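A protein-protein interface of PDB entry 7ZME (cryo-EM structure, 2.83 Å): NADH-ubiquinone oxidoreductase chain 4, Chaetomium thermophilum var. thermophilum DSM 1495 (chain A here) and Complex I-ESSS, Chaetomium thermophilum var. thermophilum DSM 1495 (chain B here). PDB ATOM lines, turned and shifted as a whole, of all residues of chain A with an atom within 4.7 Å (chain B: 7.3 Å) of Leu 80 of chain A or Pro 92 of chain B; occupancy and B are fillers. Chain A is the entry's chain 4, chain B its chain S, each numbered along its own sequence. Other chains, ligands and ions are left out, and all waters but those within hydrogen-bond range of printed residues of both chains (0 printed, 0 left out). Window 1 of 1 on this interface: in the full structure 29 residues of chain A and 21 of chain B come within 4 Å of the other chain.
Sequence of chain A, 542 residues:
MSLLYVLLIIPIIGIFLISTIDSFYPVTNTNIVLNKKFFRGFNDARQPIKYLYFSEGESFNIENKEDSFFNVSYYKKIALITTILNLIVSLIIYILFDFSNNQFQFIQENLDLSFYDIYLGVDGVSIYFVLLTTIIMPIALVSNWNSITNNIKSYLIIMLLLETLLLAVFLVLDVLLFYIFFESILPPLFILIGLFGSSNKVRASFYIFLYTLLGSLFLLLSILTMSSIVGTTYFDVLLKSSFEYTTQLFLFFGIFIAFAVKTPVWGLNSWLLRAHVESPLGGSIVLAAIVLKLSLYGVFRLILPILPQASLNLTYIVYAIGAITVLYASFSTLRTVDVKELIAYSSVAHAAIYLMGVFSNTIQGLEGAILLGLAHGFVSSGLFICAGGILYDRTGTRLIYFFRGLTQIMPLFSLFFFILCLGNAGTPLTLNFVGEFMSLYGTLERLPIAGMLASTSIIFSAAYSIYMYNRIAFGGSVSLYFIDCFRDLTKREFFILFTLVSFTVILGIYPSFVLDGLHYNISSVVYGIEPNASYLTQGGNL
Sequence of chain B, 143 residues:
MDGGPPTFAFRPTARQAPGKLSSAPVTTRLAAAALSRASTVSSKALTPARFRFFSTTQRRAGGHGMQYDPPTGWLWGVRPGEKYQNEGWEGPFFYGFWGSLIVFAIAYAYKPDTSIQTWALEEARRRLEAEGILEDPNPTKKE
CA of Gly 88 of chain B touches CE of Lys 77 of chain A (3.5 Å).
Leu 80 of chain A touches Trp 89 of chain B (CD2 to CA, 3.8 Å).
Pro 92 of chain B touches Leu 80 of chain A.
Ile 84 of chain A touches Pro 92 of chain B.
CG2 of Ile 84 of chain A touches C of Gly 96 of chain B, at 3.6 Å.
Phe 97 of chain B touches Ile 84 of chain A (N to CG2, 3.7 Å).
CD1 of Phe 93 of chain B touches CG2 of Val 142 of chain A, 3.99 Å away.
Trp 145 of chain A touches Gly 88 of chain B (CZ2 to C, 3.5 Å).
Trp 145 of chain A touches Trp 89 of chain B (CZ2 to N, 3.6 Å).
The indole nitrogen (NE1) of Trp 89 of chain B lies within hydrogen-bond range of the side-chain carboxylate (OE1) of Glu 90 of chain B, 3.2 Å away.
N of Phe 97 of chain B sits at hydrogen-bond distance from O of Pro 92 of chain B (3.1 Å).
The backbone NH (N) of Trp 98 of chain B sits at hydrogen-bond distance from the backbone carbonyl oxygen (O) of Phe 93 of chain B, 2.9 Å away.
O of Phe 97 of chain B lies within hydrogen-bond range of OG of Ser 100 of chain B.
O of Trp 145 of chain A sits at hydrogen-bond distance from NZ of Lys 76 of chain A (2.5 Å).
The backbone carbonyl oxygen (O) of Leu 80 of chain A lies within hydrogen-bond range of the side-chain hydroxyl (OG1) of Thr 83 of chain A (2.8 Å).
Of the 13 printed residues of chain A, 5 touch a printed residue of chain B.
Printed residues of chain A that touch a printed residue of chain B: Lys 77, Leu 80, Ile 84, Val 142 and Trp 145.
Hydrophobic or aromatic side chains of chain A within 4 Å of the printed part of chain B: Leu 80, Ile 84, Val 142 and Trp 145.
Along chain A the printed residues that touch a printed residue of chain B span positions 77 to 145.
Among the printed residues, 9 pairs touch across the chains.
Among the printed residues, no Asp or Glu carboxylate lies within 4 Å of a Lys or Arg side-chain nitrogen of the other chain.
Of chain B, only Trp 89 and Pro 92 come within 4 Å of Leu 80 of chain A.
Of chain A, only Leu 80 and Ile 84 come within 4 Å of Pro 92 of chain B.
No residue of chain B comes within 4 Å of Ala 79 of chain A.
Of the printed residues of chain B, Trp 145 of chain A touches Gly 88 (3.5 Å) and Trp 89 (3.6 Å).
Of the printed residues of chain A, Gly 96 of chain B touches Ile 84 (3.6 Å).
Printed residues of chain B within 4 Å of Lys 77 of chain A: Gly 88 (3.5 Å).
Lys 76 of chain A touches none of the printed residues of chain B.
Gly 91 of chain B touches none of the printed residues of chain A.
The nearest printed residue of chain B that does not touch Trp 145 of chain A is Pro 92 of chain B (6.0 Å).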
ATOM      1  N   LYS A  76       3.933 -13.854 -13.313  1.00  0.00           N
ATOM      2  CA  LYS A  76       4.291 -14.087 -14.704  1.00  0.00           C
ATOM      3  C   LYS A  76       4.142 -12.822 -15.536  1.00  0.00           C
ATOM      4  O   LYS A  76       4.922 -12.598 -16.465  1.00  0.00           O
ATOM      5  CB  LYS A  76       3.441 -15.219 -15.269  1.00  0.00           C
ATOM      6  CG  LYS A  76       3.362 -16.407 -14.343  1.00  0.00           C
ATOM      7  CD  LYS A  76       2.104 -17.213 -14.563  1.00  0.00           C
ATOM      8  CE  LYS A  76       2.107 -17.876 -15.913  1.00  0.00           C
ATOM      9  NZ  LYS A  76       1.073 -18.940 -15.993  1.00  0.00           N
ATOM     10  N   LYS A  77       3.157 -11.982 -15.214  1.00  0.00           N
ATOM     11  CA  LYS A  77       3.030 -10.702 -15.900  1.00  0.00           C
ATOM     12  C   LYS A  77       4.150  -9.750 -15.506  1.00  0.00           C
ATOM     13  O   LYS A  77       4.644  -8.988 -16.343  1.00  0.00           O
ATOM     14  CB  LYS A  77       1.666 -10.081 -15.610  1.00  0.00           C
ATOM     15  CG  LYS A  77       0.504 -10.842 -16.218  1.00  0.00           C
ATOM     16  CD  LYS A  77      -0.816 -10.158 -15.920  1.00  0.00           C
ATOM     17  CE  LYS A  77      -1.980 -10.930 -16.508  1.00  0.00           C
ATOM     18  NZ  LYS A  77      -3.288 -10.282 -16.217  1.00  0.00           N
ATOM     19  N   ILE A  78       4.560  -9.771 -14.237  1.00  0.00           N
ATOM     20  CA  ILE A  78       5.711  -8.977 -13.819  1.00  0.00           C
ATOM     21  C   ILE A  78       6.976  -9.481 -14.498  1.00  0.00           C
ATOM     22  O   ILE A  78       7.782  -8.695 -15.009  1.00  0.00           O
ATOM     23  CB  ILE A  78       5.854  -8.994 -12.286  1.00  0.00           C
ATOM     24  CG1 ILE A  78       4.648  -8.338 -11.623  1.00  0.00           C
ATOM     25  CG2 ILE A  78       7.138  -8.300 -11.855  1.00  0.00           C
ATOM     26  CD1 ILE A  78       4.721  -8.348 -10.120  1.00  0.00           C
ATOM     27  N   ALA A  79       7.173 -10.800 -14.508  1.00  0.00           N
ATOM     28  CA  ALA A  79       8.370 -11.367 -15.118  1.00  0.00           C
ATOM     29  C   ALA A  79       8.399 -11.120 -16.619  1.00  0.00           C
ATOM     30  O   ALA A  79       9.462 -10.853 -17.189  1.00  0.00           O
ATOM     31  CB  ALA A  79       8.455 -12.862 -14.816  1.00  0.00           C
ATOM     32  N   LEU A  80       7.241 -11.210 -17.278  1.00  0.00           N
ATOM     33  CA  LEU A  80       7.190 -10.955 -18.712  1.00  0.00           C
ATOM     34  C   LEU A  80       7.444  -9.488 -19.025  1.00  0.00           C
ATOM     35  O   LEU A  80       8.187  -9.169 -19.957  1.00  0.00           O
ATOM     36  CB  LEU A  80       5.845 -11.399 -19.279  1.00  0.00           C
ATOM     37  CG  LEU A  80       5.737 -11.387 -20.802  1.00  0.00           C
ATOM     38  CD1 LEU A  80       6.926 -12.097 -21.426  1.00  0.00           C
ATOM     39  CD2 LEU A  80       4.438 -12.015 -21.256  1.00  0.00           C
ATOM     40  N   ILE A  81       6.839  -8.582 -18.255  1.00  0.00           N
ATOM     41  CA  ILE A  81       7.017  -7.155 -18.505  1.00  0.00           C
ATOM     42  C   ILE A  81       8.460  -6.747 -18.247  1.00  0.00           C
ATOM     43  O   ILE A  81       9.013  -5.888 -18.944  1.00  0.00           O
ATOM     44  CB  ILE A  81       6.024  -6.341 -17.653  1.00  0.00           C
ATOM     45  CG1 ILE A  81       4.636  -6.369 -18.291  1.00  0.00           C
ATOM     46  CG2 ILE A  81       6.483  -4.906 -17.488  1.00  0.00           C
ATOM     47  CD1 ILE A  81       3.516  -6.104 -17.318  1.00  0.00           C
ATOM     48  N   THR A  82       9.094  -7.368 -17.259  1.00  0.00           N
ATOM     49  CA  THR A  82      10.506  -7.039 -16.935  1.00  0.00           C
ATOM     50  C   THR A  82      11.394  -7.346 -18.143  1.00  0.00           C
ATOM     51  O   THR A  82      12.178  -6.469 -18.527  1.00  0.00           O
ATOM     52  CB  THR A  82      10.942  -7.762 -15.658  1.00  0.00           C
ATOM     53  OG1 THR A  82      10.128  -7.267 -14.594  1.00  0.00           O
ATOM     54  CG2 THR A  82      12.405  -7.573 -15.331  1.00  0.00           C
ATOM     55  N   THR A  83      11.252  -8.529 -18.734  1.00  0.00           N
ATOM     56  CA  THR A  83      12.085  -8.952 -19.889  1.00  0.00           C
ATOM     57  C   THR A  83      11.835  -8.054 -21.104  1.00  0.00           C
ATOM     58  O   THR A  83      12.749  -7.898 -21.910  1.00  0.00           O
ATOM     59  CB  THR A  83      11.908 -10.448 -20.181  1.00  0.00           C
ATOM     60  OG1 THR A  83      10.514 -10.758 -20.159  1.00  0.00           O
ATOM     61  CG2 THR A  83      12.643 -11.332 -19.200  1.00  0.00           C
ATOM     62  N   ILE A  84      10.637  -7.501 -21.245  1.00  0.00           N
ATOM     63  CA  ILE A  84      10.334  -6.715 -22.471  1.00  0.00           C
ATOM     64  C   ILE A  84      10.924  -5.330 -22.278  1.00  0.00           C
ATOM     65  O   ILE A  84      11.471  -4.793 -23.239  1.00  0.00           O
ATOM     66  CB  ILE A  84       8.811  -6.682 -22.720  1.00  0.00           C
ATOM     67  CG1 ILE A  84       8.297  -8.058 -23.148  1.00  0.00           C
ATOM     68  CG2 ILE A  84       8.439  -5.610 -23.730  1.00  0.00           C
ATOM     69  CD1 ILE A  84       6.833  -8.264 -22.884  1.00  0.00           C
ATOM     70  N   PRO A 138      11.957 -13.111 -23.102  1.00  0.00           N
ATOM     71  CA  PRO A 138      10.509 -13.012 -23.047  1.00  0.00           C
ATOM     72  C   PRO A 138       9.866 -14.271 -23.640  1.00  0.00           C
ATOM     73  O   PRO A 138       8.928 -14.751 -23.063  1.00  0.00           O
ATOM     74  CB  PRO A 138      10.226 -11.796 -23.939  1.00  0.00           C
ATOM     75  CG  PRO A 138      11.465 -10.958 -23.838  1.00  0.00           C
ATOM     76  CD  PRO A 138      12.565 -11.990 -23.819  1.00  0.00           C
ATOM     77  N   LEU A 141       9.952 -17.279 -21.253  1.00  0.00           N
ATOM     78  CA  LEU A 141       8.907 -17.169 -20.209  1.00  0.00           C
ATOM     79  C   LEU A 141       7.530 -17.510 -20.790  1.00  0.00           C
ATOM     80  O   LEU A 141       6.822 -18.295 -20.176  1.00  0.00           O
ATOM     81  CB  LEU A 141       8.951 -15.758 -19.618  1.00  0.00           C
ATOM     82  CG  LEU A 141      10.190 -15.435 -18.791  1.00  0.00           C
ATOM     83  CD1 LEU A 141      10.162 -13.990 -18.331  1.00  0.00           C
ATOM     84  CD2 LEU A 141      10.305 -16.375 -17.604  1.00  0.00           C
ATOM     85  N   VAL A 142       7.151 -16.937 -21.927  1.00  0.00           N
ATOM     86  CA  VAL A 142       5.818 -17.195 -22.555  1.00  0.00           C
ATOM     87  C   VAL A 142       5.726 -18.663 -22.969  1.00  0.00           C
ATOM     88  O   VAL A 142       4.639 -19.200 -22.907  1.00  0.00           O
ATOM     89  CB  VAL A 142       5.569 -16.244 -23.736  1.00  0.00           C
ATOM     90  CG1 VAL A 142       4.204 -16.447 -24.367  1.00  0.00           C
ATOM     91  CG2 VAL A 142       5.738 -14.792 -23.340  1.00  0.00           C
ATOM     92  N   TRP A 145       4.551 -20.703 -19.970  1.00  0.00           N
ATOM     93  CA  TRP A 145       3.485 -19.966 -19.246  1.00  0.00           C
ATOM     94  C   TRP A 145       2.544 -20.910 -18.502  1.00  0.00           C
ATOM     95  O   TRP A 145       2.230 -20.625 -17.363  1.00  0.00           O
ATOM     96  CB  TRP A 145       2.726 -19.088 -20.242  1.00  0.00           C
ATOM     97  CG  TRP A 145       1.890 -17.994 -19.652  1.00  0.00           C
ATOM     98  CD1 TRP A 145       0.558 -18.041 -19.359  1.00  0.00           C
ATOM     99  CD2 TRP A 145       2.321 -16.660 -19.327  1.00  0.00           C
ATOM    100  NE1 TRP A 145       0.139 -16.840 -18.856  1.00  0.00           N
ATOM    101  CE2 TRP A 145       1.197 -15.975 -18.822  1.00  0.00           C
ATOM    102  CE3 TRP A 145       3.542 -15.984 -19.404  1.00  0.00           C
ATOM    103  CZ2 TRP A 145       1.264 -14.652 -18.393  1.00  0.00           C
ATOM    104  CZ3 TRP A 145       3.606 -14.678 -18.981  1.00  0.00           C
ATOM    105  CH2 TRP A 145       2.480 -14.020 -18.489  1.00  0.00           C
ATOM    106  N   GLY B  88      -3.038 -13.757 -20.174  1.00  0.00           N
ATOM    107  CA  GLY B  88      -2.151 -12.850 -19.429  1.00  0.00           C
ATOM    108  C   GLY B  88      -0.856 -12.498 -20.150  1.00  0.00           C
ATOM    109  O   GLY B  88      -0.215 -11.522 -19.736  1.00  0.00           O
ATOM    110  N   TRP B  89      -0.494 -13.195 -21.213  1.00  0.00           N
ATOM    111  CA  TRP B  89       0.758 -12.908 -21.944  1.00  0.00           C
ATOM    112  C   TRP B  89       0.471 -12.073 -23.182  1.00  0.00           C
ATOM    113  O   TRP B  89       1.436 -11.604 -23.772  1.00  0.00           O
ATOM    114  CB  TRP B  89       1.378 -14.247 -22.382  1.00  0.00           C
ATOM    115  CG  TRP B  89       0.489 -14.999 -23.327  1.00  0.00           C
ATOM    116  CD1 TRP B  89      -0.433 -15.945 -22.996  1.00  0.00           C
ATOM    117  CD2 TRP B  89       0.393 -14.838 -24.758  1.00  0.00           C
ATOM    118  NE1 TRP B  89      -1.085 -16.389 -24.112  1.00  0.00           N
ATOM    119  CE2 TRP B  89      -0.603 -15.726 -25.206  1.00  0.00           C
ATOM    120  CE3 TRP B  89       1.050 -14.040 -25.702  1.00  0.00           C
ATOM    121  CZ2 TRP B  89      -0.957 -15.830 -26.548  1.00  0.00           C
ATOM    122  CZ3 TRP B  89       0.699 -14.141 -27.028  1.00  0.00           C
ATOM    123  CH2 TRP B  89      -0.288 -15.032 -27.444  1.00  0.00           C
ATOM    124  N   GLU B  90      -0.793 -11.824 -23.519  1.00  0.00           N
ATOM    125  CA  GLU B  90      -1.095 -11.280 -24.841  1.00  0.00           C
ATOM    126  C   GLU B  90      -0.764  -9.799 -24.931  1.00  0.00           C
ATOM    127  O   GLU B  90      -0.153  -9.350 -25.906  1.00  0.00           O
ATOM    128  CB  GLU B  90      -2.564 -11.522 -25.172  1.00  0.00           C
ATOM    129  CG  GLU B  90      -2.896 -12.970 -25.449  1.00  0.00           C
ATOM    130  CD  GLU B  90      -3.309 -13.722 -24.199  1.00  0.00           C
ATOM    131  OE1 GLU B  90      -3.854 -14.834 -24.331  1.00  0.00           O
ATOM    132  OE2 GLU B  90      -3.088 -13.207 -23.088  1.00  0.00           O
ATOM    133  N   GLY B  91      -1.172  -9.022 -23.934  1.00  0.00           N
ATOM    134  CA  GLY B  91      -0.904  -7.605 -23.916  1.00  0.00           C
ATOM    135  C   GLY B  91       0.576  -7.290 -23.904  1.00  0.00           C
ATOM    136  O   GLY B  91       1.070  -6.502 -24.714  1.00  0.00           O
ATOM    137  N   PRO B  92       1.320  -7.899 -22.975  1.00  0.00           N
ATOM    138  CA  PRO B  92       2.776  -7.714 -22.992  1.00  0.00           C
ATOM    139  C   PRO B  92       3.443  -8.167 -24.279  1.00  0.00           C
ATOM    140  O   PRO B  92       4.386  -7.514 -24.738  1.00  0.00           O
ATOM    141  CB  PRO B  92       3.230  -8.543 -21.786  1.00  0.00           C
ATOM    142  CG  PRO B  92       2.093  -8.483 -20.862  1.00  0.00           C
ATOM    143  CD  PRO B  92       0.874  -8.537 -21.725  1.00  0.00           C
ATOM    144  N   PHE B  93       2.991  -9.267 -24.880  1.00  0.00           N
ATOM    145  CA  PHE B  93       3.659  -9.765 -26.077  1.00  0.00           C
ATOM    146  C   PHE B  93       3.361  -8.895 -27.291  1.00  0.00           C
ATOM    147  O   PHE B  93       4.267  -8.545 -28.053  1.00  0.00           O
ATOM    148  CB  PHE B  93       3.257 -11.214 -26.345  1.00  0.00           C
ATOM    149  CG  PHE B  93       4.280 -11.988 -27.118  1.00  0.00           C
ATOM    150  CD1 PHE B  93       5.449 -12.403 -26.518  1.00  0.00           C
ATOM    151  CD2 PHE B  93       4.073 -12.295 -28.452  1.00  0.00           C
ATOM    152  CE1 PHE B  93       6.388 -13.111 -27.227  1.00  0.00           C
ATOM    153  CE2 PHE B  93       5.008 -13.002 -29.164  1.00  0.00           C
ATOM    154  CZ  PHE B  93       6.168 -13.408 -28.551  1.00  0.00           C
ATOM    155  N   PHE B  94       2.096  -8.527 -27.485  1.00  0.00           N
ATOM    156  CA  PHE B  94       1.732  -7.797 -28.693  1.00  0.00           C
ATOM    157  C   PHE B  94       2.055  -6.313 -28.569  1.00  0.00           C
ATOM    158  O   PHE B  94       2.712  -5.740 -29.442  1.00  0.00           O
ATOM    159  CB  PHE B  94       0.252  -8.005 -29.006  1.00  0.00           C
ATOM    160  CG  PHE B  94      -0.092  -9.419 -29.363  1.00  0.00           C
ATOM    161  CD1 PHE B  94       0.730 -10.154 -30.193  1.00  0.00           C
ATOM    162  CD2 PHE B  94      -1.235 -10.012 -28.868  1.00  0.00           C
ATOM    163  CE1 PHE B  94       0.418 -11.451 -30.521  1.00  0.00           C
ATOM    164  CE2 PHE B  94      -1.550 -11.310 -29.195  1.00  0.00           C
ATOM    165  CZ  PHE B  94      -0.725 -12.029 -30.020  1.00  0.00           C
ATOM    166  N   TYR B  95       1.601  -5.675 -27.492  1.00  0.00           N
ATOM    167  CA  TYR B  95       1.856  -4.249 -27.331  1.00  0.00           C
ATOM    168  C   TYR B  95       3.283  -3.967 -26.883  1.00  0.00           C
ATOM    169  O   TYR B  95       3.852  -2.940 -27.268  1.00  0.00           O
ATOM    170  CB  TYR B  95       0.866  -3.641 -26.336  1.00  0.00           C
ATOM    171  CG  TYR B  95      -0.588  -3.801 -26.726  1.00  0.00           C
ATOM    172  CD1 TYR B  95      -0.960  -3.945 -28.054  1.00  0.00           C
ATOM    173  CD2 TYR B  95      -1.586  -3.809 -25.763  1.00  0.00           C
ATOM    174  CE1 TYR B  95      -2.283  -4.091 -28.414  1.00  0.00           C
ATOM    175  CE2 TYR B  95      -2.915  -3.956 -26.112  1.00  0.00           C
ATOM    176  CZ  TYR B  95      -3.257  -4.096 -27.439  1.00  0.00           C
ATOM    177  OH  TYR B  95      -4.577  -4.242 -27.795  1.00  0.00           O
ATOM    178  N   GLY B  96       3.897  -4.894 -26.147  1.00  0.00           N
ATOM    179  CA  GLY B  96       5.278  -4.675 -25.689  1.00  0.00           C
ATOM    180  C   GLY B  96       6.348  -5.199 -26.623  1.00  0.00           C
ATOM    181  O   GLY B  96       6.994  -4.382 -27.267  1.00  0.00           O
ATOM    182  N   PHE B  97       6.509  -6.522 -26.708  1.00  0.00           N
ATOM    183  CA  PHE B  97       7.617  -7.121 -27.488  1.00  0.00           C
ATOM    184  C   PHE B  97       7.468  -6.819 -28.976  1.00  0.00           C
ATOM    185  O   PHE B  97       8.396  -6.258 -29.571  1.00  0.00           O
ATOM    186  CB  PHE B  97       7.522  -8.635 -27.291  1.00  0.00           C
ATOM    187  CG  PHE B  97       8.507  -9.497 -28.037  1.00  0.00           C
ATOM    188  CD1 PHE B  97       9.759  -9.760 -27.512  1.00  0.00           C
ATOM    189  CD2 PHE B  97       8.157 -10.094 -29.235  1.00  0.00           C
ATOM    190  CE1 PHE B  97      10.656 -10.568 -28.188  1.00  0.00           C
ATOM    191  CE2 PHE B  97       9.057 -10.897 -29.912  1.00  0.00           C
ATOM    192  CZ  PHE B  97      10.305 -11.135 -29.389  1.00  0.00           C
ATOM    193  N   TRP B  98       6.302  -7.133 -29.539  1.00  0.00           N
ATOM    194  CA  TRP B  98       6.101  -6.915 -30.990  1.00  0.00           C
ATOM    195  C   TRP B  98       6.013  -5.424 -31.269  1.00  0.00           C
ATOM    196  O   TRP B  98       6.648  -4.982 -32.218  1.00  0.00           O
ATOM    197  CB  TRP B  98       4.896  -7.692 -31.517  1.00  0.00           C
ATOM    198  CG  TRP B  98       5.280  -8.997 -32.136  1.00  0.00           C
ATOM    199  CD1 TRP B  98       5.046 -10.243 -31.636  1.00  0.00           C
ATOM    200  CD2 TRP B  98       5.994  -9.185 -33.369  1.00  0.00           C
ATOM    201  NE1 TRP B  98       5.549 -11.192 -32.481  1.00  0.00           N
ATOM    202  CE2 TRP B  98       6.144 -10.575 -33.549  1.00  0.00           C
ATOM    203  CE3 TRP B  98       6.516  -8.320 -34.336  1.00  0.00           C
ATOM    204  CZ2 TRP B  98       6.790 -11.117 -34.659  1.00  0.00           C
ATOM    205  CZ3 TRP B  98       7.154  -8.857 -35.431  1.00  0.00           C
ATOM    206  CH2 TRP B  98       7.288 -10.236 -35.588  1.00  0.00           C
ATOM    207  N   GLY B  99       5.300  -4.685 -30.413  1.00  0.00           N
ATOM    208  CA  GLY B  99       5.122  -3.241 -30.634  1.00  0.00           C
ATOM    209  C   GLY B  99       6.454  -2.532 -30.610  1.00  0.00           C
ATOM    210  O   GLY B  99       6.683  -1.708 -31.496  1.00  0.00           O
ATOM    211  N   SER B 100       7.319  -2.888 -29.659  1.00  0.00           N
ATOM    212  CA  SER B 100       8.663  -2.271 -29.559  1.00  0.00           C
ATOM    213  C   SER B 100       9.471  -2.617 -30.800  1.00  0.00           C
ATOM    214  O   SER B 100      10.183  -1.734 -31.283  1.00  0.00           O
ATOM    215  CB  SER B 100       9.378  -2.731 -28.330  1.00  0.00           C
ATOM    216  OG  SER B 100       9.623  -4.122 -28.386  1.00  0.00           O
